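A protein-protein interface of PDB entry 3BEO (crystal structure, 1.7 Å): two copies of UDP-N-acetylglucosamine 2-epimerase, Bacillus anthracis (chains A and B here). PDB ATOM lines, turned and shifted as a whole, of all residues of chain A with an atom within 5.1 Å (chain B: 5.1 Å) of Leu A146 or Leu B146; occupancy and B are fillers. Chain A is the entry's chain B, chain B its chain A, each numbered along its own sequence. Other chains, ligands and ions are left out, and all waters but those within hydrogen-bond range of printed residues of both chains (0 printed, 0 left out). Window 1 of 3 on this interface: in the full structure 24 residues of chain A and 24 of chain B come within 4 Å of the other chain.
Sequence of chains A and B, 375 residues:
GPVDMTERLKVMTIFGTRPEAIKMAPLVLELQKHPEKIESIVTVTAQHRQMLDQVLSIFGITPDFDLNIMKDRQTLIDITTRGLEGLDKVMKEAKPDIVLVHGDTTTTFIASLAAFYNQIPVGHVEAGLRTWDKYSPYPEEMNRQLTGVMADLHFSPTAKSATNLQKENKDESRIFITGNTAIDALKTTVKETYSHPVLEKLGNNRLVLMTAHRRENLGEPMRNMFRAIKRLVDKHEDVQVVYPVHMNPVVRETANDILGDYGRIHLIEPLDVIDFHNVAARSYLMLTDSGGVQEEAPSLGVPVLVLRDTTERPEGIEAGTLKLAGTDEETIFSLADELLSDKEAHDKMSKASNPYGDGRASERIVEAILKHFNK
Phe A109 touches its own counterpart, Phe B109. Gln A145 touches Val B149, and with the chains exchanged Val A149 touches Gln B145. Leu A146 touches Val B149, and with the chains exchanged Val A149 touches Leu B146. Leu A146 touches Met B150, and with the chains exchanged Met A150 touches Leu B146. 11 positions are printed for both chains. Of the 14 pairs that touch across the chains among the printed residues, 14 have their exchanged pair printed and touching as well.
SD of Met A142 lies close to O of Val B149 (3.6 Å). The backbone carbonyl oxygen (O) of Val A149 sits close to the side-chain sulfur (SD) of Met B142 (3.4 Å).
Among the printed residues, merely in contact across the chains: Phe A109 with Phe B109, Phe A109 with Leu B113, Leu A113 with Phe B109, Met A142 with Met B150, Gln A145 with Val B149, Leu A146 with Leu B146, Leu A146 with Val B149, Leu A146 with Met B150, Val A149 with Gln B145, Val A149 with Leu B146, Met A150 with Met B142 and Met A150 with Leu B146.
Printed residues of chain B within 4 Å of Gln A145: Val B149. Of chain B, only Leu B146 (3.5 Å), Val B149 (3.8 Å) and Met B150 (3.97 Å) come within 4 Å of Leu A146. Of the printed residues of chain A, Phe B109 touches Phe A109 (3.7 Å) and Leu A113 (3.8 Å). Printed residues of chain A within 4 Å of Gln B145: Val A149 (3.98 Å). Of the printed residues of chain A, Leu B146 touches Leu A146, Val A149 and Met A150. The nearest residue of chain B that does not touch Leu A146 is Leu B113 (4.2 Å). The nearest residue of chain A that does not touch Leu B146 is Leu A113 (4.3 Å).
Hydrophobic or aromatic side chains of chain B within 4 Å of the printed part of chain A: Phe B109, Leu B113, Met B142, Leu B146, Val B149 and Met B150. Of the 11 printed residues of chain A, 7 touch a printed residue of chain B. Hydrophobic or aromatic side chains of chain A within 4 Å of the printed part of chain B: Phe A109, Leu A113, Met A142, Leu A146, Val A149 and Met A150.
The side-chain sulfur (SD) of Met B150 sits at hydrogen-bond distance from the backbone NH (N) of Leu B113 (3.6 Å). The backbone NH (N) of Leu A113 sits close to the side-chain sulfur (SD) of Met A150, at 3.7 Å.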
ATOM      1  N   PHE A 109     -12.375  -6.075  36.074  1.00  0.00           N
ATOM      2  CA  PHE A 109     -12.998  -5.877  34.754  1.00  0.00           C
ATOM      3  C   PHE A 109     -14.089  -4.820  34.798  1.00  0.00           C
ATOM      4  O   PHE A 109     -14.010  -3.852  34.027  1.00  0.00           O
ATOM      5  CB  PHE A 109     -13.482  -7.227  34.205  1.00  0.00           C
ATOM      6  CG  PHE A 109     -14.565  -7.128  33.163  1.00  0.00           C
ATOM      7  CD1 PHE A 109     -14.350  -6.402  32.032  1.00  0.00           C
ATOM      8  CD2 PHE A 109     -15.775  -7.809  33.304  1.00  0.00           C
ATOM      9  CE1 PHE A 109     -15.325  -6.310  31.061  1.00  0.00           C
ATOM     10  CE2 PHE A 109     -16.745  -7.721  32.324  1.00  0.00           C
ATOM     11  CZ  PHE A 109     -16.521  -6.934  31.239  1.00  0.00           C
ATOM     12  N   LEU A 113     -14.334  -1.060  33.157  1.00  0.00           N
ATOM     13  CA  LEU A 113     -15.456  -0.752  32.264  1.00  0.00           C
ATOM     14  C   LEU A 113     -16.200   0.512  32.715  1.00  0.00           C
ATOM     15  O   LEU A 113     -16.453   1.419  31.924  1.00  0.00           O
ATOM     16  CB  LEU A 113     -16.445  -1.913  32.157  1.00  0.00           C
ATOM     17  CG  LEU A 113     -17.471  -1.880  31.031  1.00  0.00           C
ATOM     18  CD1 LEU A 113     -16.768  -1.919  29.630  1.00  0.00           C
ATOM     19  CD2 LEU A 113     -18.460  -2.992  31.140  1.00  0.00           C
ATOM     20  N   MET A 142      -9.620 -14.035  31.045  1.00  0.00           N
ATOM     21  CA  MET A 142     -10.409 -13.101  30.268  1.00  0.00           C
ATOM     22  C   MET A 142     -10.473 -11.774  30.992  1.00  0.00           C
ATOM     23  O   MET A 142     -10.303 -10.726  30.349  1.00  0.00           O
ATOM     24  CB  MET A 142     -11.780 -13.663  29.955  1.00  0.00           C
ATOM     25  CG  MET A 142     -12.490 -12.896  28.838  1.00  0.00           C
ATOM     26  SD  MET A 142     -11.557 -12.876  27.332  1.00  0.00           S
ATOM     27  CE  MET A 142     -11.481 -14.557  26.801  1.00  0.00           C
ATOM     28  N   ASN A 143     -10.575 -11.801  32.323  1.00  0.00           N
ATOM     29  CA  ASN A 143     -10.682 -10.520  33.009  1.00  0.00           C
ATOM     30  C   ASN A 143      -9.435  -9.653  32.759  1.00  0.00           C
ATOM     31  O   ASN A 143      -9.505  -8.446  32.557  1.00  0.00           O
ATOM     32  CB  ASN A 143     -10.920 -10.714  34.519  1.00  0.00           C
ATOM     33  CG  ASN A 143     -12.303 -11.190  34.839  1.00  0.00           C
ATOM     34  OD1 ASN A 143     -13.256 -10.977  34.048  1.00  0.00           O
ATOM     35  ND2 ASN A 143     -12.445 -11.892  35.995  1.00  0.00           N
ATOM     36  N   ARG A 144      -8.248 -10.242  32.867  1.00  0.00           N
ATOM     37  CA  ARG A 144      -6.982  -9.501  32.671  1.00  0.00           C
ATOM     38  C   ARG A 144      -6.790  -9.122  31.186  1.00  0.00           C
ATOM     39  O   ARG A 144      -6.206  -8.086  30.900  1.00  0.00           O
ATOM     40  CB  ARG A 144      -5.751 -10.233  33.314  1.00  0.00           C
ATOM     41  CG  ARG A 144      -5.484 -11.627  32.807  1.00  0.00           C
ATOM     42  CD  ARG A 144      -4.844 -12.441  33.872  1.00  0.00           C
ATOM     43  NE  ARG A 144      -4.625 -13.831  33.437  1.00  0.00           N
ATOM     44  CZ  ARG A 144      -4.401 -14.839  34.289  1.00  0.00           C
ATOM     45  NH1 ARG A 144      -4.351 -14.605  35.584  1.00  0.00           N
ATOM     46  NH2 ARG A 144      -4.185 -16.089  33.835  1.00  0.00           N
ATOM     47  N   GLN A 145      -7.346  -9.901  30.240  1.00  0.00           N
ATOM     48  CA  GLN A 145      -7.299  -9.505  28.832  1.00  0.00           C
ATOM     49  C   GLN A 145      -8.198  -8.309  28.529  1.00  0.00           C
ATOM     50  O   GLN A 145      -7.815  -7.354  27.800  1.00  0.00           O
ATOM     51  CB  GLN A 145      -7.714 -10.686  27.940  1.00  0.00           C
ATOM     52  CG  GLN A 145      -6.599 -11.689  27.802  1.00  0.00           C
ATOM     53  CD  GLN A 145      -5.593 -11.383  26.657  1.00  0.00           C
ATOM     54  OE1 GLN A 145      -5.433 -10.237  26.184  1.00  0.00           O
ATOM     55  NE2 GLN A 145      -4.954 -12.429  26.192  1.00  0.00           N
ATOM     56  N   LEU A 146      -9.401  -8.394  29.069  1.00  0.00           N
ATOM     57  CA  LEU A 146     -10.402  -7.331  28.954  1.00  0.00           C
ATOM     58  C   LEU A 146      -9.876  -6.020  29.567  1.00  0.00           C
ATOM     59  O   LEU A 146      -9.823  -4.975  28.898  1.00  0.00           O
ATOM     60  CB  LEU A 146     -11.710  -7.768  29.592  1.00  0.00           C
ATOM     61  CG  LEU A 146     -12.535  -8.907  28.950  1.00  0.00           C
ATOM     62  CD1 LEU A 146     -13.592  -9.501  29.869  1.00  0.00           C
ATOM     63  CD2 LEU A 146     -13.157  -8.380  27.704  1.00  0.00           C
ATOM     64  N   THR A 147      -9.489  -6.076  30.840  1.00  0.00           N
ATOM     65  CA  THR A 147      -8.817  -4.990  31.542  1.00  0.00           C
ATOM     66  C   THR A 147      -7.600  -4.463  30.741  1.00  0.00           C
ATOM     67  O   THR A 147      -7.477  -3.236  30.534  1.00  0.00           O
ATOM     68  CB  THR A 147      -8.373  -5.451  32.981  1.00  0.00           C
ATOM     69  OG1 THR A 147      -9.511  -5.859  33.757  1.00  0.00           O
ATOM     70  CG2 THR A 147      -7.655  -4.319  33.663  1.00  0.00           C
ATOM     71  N   GLY A 148      -6.846  -5.360  30.087  1.00  0.00           N
ATOM     72  CA  GLY A 148      -5.675  -4.972  29.270  1.00  0.00           C
ATOM     73  C   GLY A 148      -5.961  -4.036  28.117  1.00  0.00           C
ATOM     74  O   GLY A 148      -5.163  -3.060  27.884  1.00  0.00           O
ATOM     75  N   VAL A 149      -7.070  -4.299  27.403  1.00  0.00           N
ATOM     76  CA  VAL A 149      -7.467  -3.419  26.283  1.00  0.00           C
ATOM     77  C   VAL A 149      -8.048  -2.084  26.730  1.00  0.00           C
ATOM     78  O   VAL A 149      -8.022  -1.099  25.945  1.00  0.00           O
ATOM     79  CB  VAL A 149      -8.357  -4.123  25.249  1.00  0.00           C
ATOM     80  CG1 VAL A 149      -7.531  -5.219  24.549  1.00  0.00           C
ATOM     81  CG2 VAL A 149      -9.603  -4.614  25.832  1.00  0.00           C
ATOM     82  N   MET A 150      -8.541  -2.066  27.972  1.00  0.00           N
ATOM     83  CA  MET A 150      -9.086  -0.856  28.593  1.00  0.00           C
ATOM     84  C   MET A 150      -8.022   0.045  29.217  1.00  0.00           C
ATOM     85  O   MET A 150      -8.197   1.218  29.249  1.00  0.00           O
ATOM     86  CB  MET A 150     -10.205  -1.189  29.578  1.00  0.00           C
ATOM     87  CG  MET A 150     -11.493  -1.567  28.830  1.00  0.00           C
ATOM     88  SD  MET A 150     -12.945  -1.812  29.832  1.00  0.00           S
ATOM     89  CE  MET A 150     -12.553  -3.418  30.529  1.00  0.00           C
ATOM     90  N   PHE B 109     -20.499  -6.555  22.273  1.00  0.00           N
ATOM     91  CA  PHE B 109     -19.706  -6.770  23.471  1.00  0.00           C
ATOM     92  C   PHE B 109     -20.465  -7.611  24.460  1.00  0.00           C
ATOM     93  O   PHE B 109     -19.907  -8.603  24.946  1.00  0.00           O
ATOM     94  CB  PHE B 109     -19.270  -5.417  24.060  1.00  0.00           C
ATOM     95  CG  PHE B 109     -18.884  -5.448  25.516  1.00  0.00           C
ATOM     96  CD1 PHE B 109     -17.935  -6.326  25.976  1.00  0.00           C
ATOM     97  CD2 PHE B 109     -19.475  -4.595  26.409  1.00  0.00           C
ATOM     98  CE1 PHE B 109     -17.559  -6.328  27.344  1.00  0.00           C
ATOM     99  CE2 PHE B 109     -19.097  -4.586  27.756  1.00  0.00           C
ATOM    100  CZ  PHE B 109     -18.163  -5.485  28.207  1.00  0.00           C
ATOM    101  N   LEU B 113     -19.668 -11.360  25.892  1.00  0.00           N
ATOM    102  CA  LEU B 113     -19.544 -11.584  27.340  1.00  0.00           C
ATOM    103  C   LEU B 113     -20.506 -12.711  27.861  1.00  0.00           C
ATOM    104  O   LEU B 113     -20.110 -13.598  28.580  1.00  0.00           O
ATOM    105  CB  LEU B 113     -19.760 -10.297  28.100  1.00  0.00           C
ATOM    106  CG  LEU B 113     -19.230 -10.258  29.534  1.00  0.00           C
ATOM    107  CD1 LEU B 113     -17.719 -10.450  29.562  1.00  0.00           C
ATOM    108  CD2 LEU B 113     -19.716  -9.000  30.283  1.00  0.00           C
ATOM    109  N   MET B 142     -13.465   0.385  21.610  1.00  0.00           N
ATOM    110  CA  MET B 142     -13.331  -0.508  22.744  1.00  0.00           C
ATOM    111  C   MET B 142     -14.210  -1.737  22.562  1.00  0.00           C
ATOM    112  O   MET B 142     -13.777  -2.825  22.879  1.00  0.00           O
ATOM    113  CB  MET B 142     -13.634   0.208  24.063  1.00  0.00           C
ATOM    114  CG  MET B 142     -13.124  -0.524  25.259  1.00  0.00           C
ATOM    115  SD  MET B 142     -11.364  -0.793  25.186  1.00  0.00           S
ATOM    116  CE  MET B 142     -10.708   0.820  25.161  1.00  0.00           C
ATOM    117  N   ASN B 143     -15.415  -1.582  22.018  1.00  0.00           N
ATOM    118  CA  ASN B 143     -16.313  -2.774  21.879  1.00  0.00           C
ATOM    119  C   ASN B 143     -15.683  -3.860  20.981  1.00  0.00           C
ATOM    120  O   ASN B 143     -15.725  -5.020  21.300  1.00  0.00           O
ATOM    121  CB  ASN B 143     -17.663  -2.384  21.285  1.00  0.00           C
ATOM    122  CG  ASN B 143     -18.538  -1.622  22.258  1.00  0.00           C
ATOM    123  OD1 ASN B 143     -18.360  -1.717  23.502  1.00  0.00           O
ATOM    124  ND2 ASN B 143     -19.498  -0.839  21.707  1.00  0.00           N
ATOM    125  N   ARG B 144     -15.077  -3.447  19.883  1.00  0.00           N
ATOM    126  CA  ARG B 144     -14.423  -4.414  18.962  1.00  0.00           C
ATOM    127  C   ARG B 144     -13.107  -4.934  19.558  1.00  0.00           C
ATOM    128  O   ARG B 144     -12.772  -6.069  19.355  1.00  0.00           O
ATOM    129  CB  ARG B 144     -14.290  -3.816  17.540  1.00  0.00           C
ATOM    130  CG  ARG B 144     -13.483  -2.599  17.385  1.00  0.00           C
ATOM    131  CD  ARG B 144     -13.931  -1.772  16.189  1.00  0.00           C
ATOM    132  NE  ARG B 144     -13.233  -0.501  16.067  1.00  0.00           N
ATOM    133  CZ  ARG B 144     -13.676   0.543  15.381  1.00  0.00           C
ATOM    134  NH1 ARG B 144     -14.848   0.457  14.783  1.00  0.00           N
ATOM    135  NH2 ARG B 144     -12.968   1.684  15.277  1.00  0.00           N
ATOM    136  N   GLN B 145     -12.403  -4.158  20.385  1.00  0.00           N
ATOM    137  CA  GLN B 145     -11.236  -4.736  21.137  1.00  0.00           C
ATOM    138  C   GLN B 145     -11.606  -5.784  22.192  1.00  0.00           C
ATOM    139  O   GLN B 145     -10.929  -6.870  22.356  1.00  0.00           O
ATOM    140  CB  GLN B 145     -10.468  -3.623  21.827  1.00  0.00           C
ATOM    141  CG  GLN B 145      -9.616  -2.801  20.805  1.00  0.00           C
ATOM    142  CD  GLN B 145      -8.240  -3.400  20.563  1.00  0.00           C
ATOM    143  OE1 GLN B 145      -8.008  -4.644  20.643  1.00  0.00           O
ATOM    144  NE2 GLN B 145      -7.320  -2.541  20.204  1.00  0.00           N
ATOM    145  N   LEU B 146     -12.645  -5.446  22.935  1.00  0.00           N
ATOM    146  CA  LEU B 146     -13.153  -6.332  23.999  1.00  0.00           C
ATOM    147  C   LEU B 146     -13.646  -7.652  23.384  1.00  0.00           C
ATOM    148  O   LEU B 146     -13.281  -8.760  23.801  1.00  0.00           O
ATOM    149  CB  LEU B 146     -14.300  -5.623  24.733  1.00  0.00           C
ATOM    150  CG  LEU B 146     -13.895  -4.468  25.686  1.00  0.00           C
ATOM    151  CD1 LEU B 146     -15.092  -3.636  26.021  1.00  0.00           C
ATOM    152  CD2 LEU B 146     -13.170  -4.957  26.918  1.00  0.00           C
ATOM    153  N   THR B 147     -14.531  -7.501  22.401  1.00  0.00           N
ATOM    154  CA  THR B 147     -15.033  -8.628  21.558  1.00  0.00           C
ATOM    155  C   THR B 147     -13.820  -9.447  20.982  1.00  0.00           C
ATOM    156  O   THR B 147     -13.831 -10.714  21.039  1.00  0.00           O
ATOM    157  CB  THR B 147     -15.998  -8.134  20.433  1.00  0.00           C
ATOM    158  OG1 THR B 147     -17.165  -7.551  20.976  1.00  0.00           O
ATOM    159  CG2 THR B 147     -16.461  -9.271  19.610  1.00  0.00           C
ATOM    160  N   GLY B 148     -12.782  -8.752  20.497  1.00  0.00           N
ATOM    161  CA  GLY B 148     -11.534  -9.358  19.943  1.00  0.00           C
ATOM    162  C   GLY B 148     -10.887 -10.363  20.868  1.00  0.00           C
ATOM    163  O   GLY B 148     -10.486 -11.439  20.455  1.00  0.00           O
ATOM    164  N   VAL B 149     -10.755  -9.985  22.133  1.00  0.00           N
ATOM    165  CA  VAL B 149     -10.132 -10.927  23.107  1.00  0.00           C
ATOM    166  C   VAL B 149     -11.011 -12.099  23.517  1.00  0.00           C
ATOM    167  O   VAL B 149     -10.484 -13.161  23.909  1.00  0.00           O
ATOM    168  CB  VAL B 149      -9.567 -10.134  24.307  1.00  0.00           C
ATOM    169  CG1 VAL B 149      -8.459  -9.219  23.841  1.00  0.00           C
ATOM    170  CG2 VAL B 149     -10.633  -9.478  25.098  1.00  0.00           C
ATOM    171  N   MET B 150     -12.328 -11.938  23.357  1.00  0.00           N
ATOM    172  CA  MET B 150     -13.317 -13.019  23.633  1.00  0.00           C
ATOM    173  C   MET B 150     -13.552 -13.987  22.467  1.00  0.00           C
ATOM    174  O   MET B 150     -13.889 -15.144  22.689  1.00  0.00           O
ATOM    175  CB  MET B 150     -14.650 -12.429  24.120  1.00  0.00           C
ATOM    176  CG  MET B 150     -14.521 -11.864  25.533  1.00  0.00           C
ATOM    177  SD  MET B 150     -16.056 -11.269  26.212  1.00  0.00           S
ATOM    178  CE  MET B 150     -16.068  -9.698  25.346  1.00  0.00           C
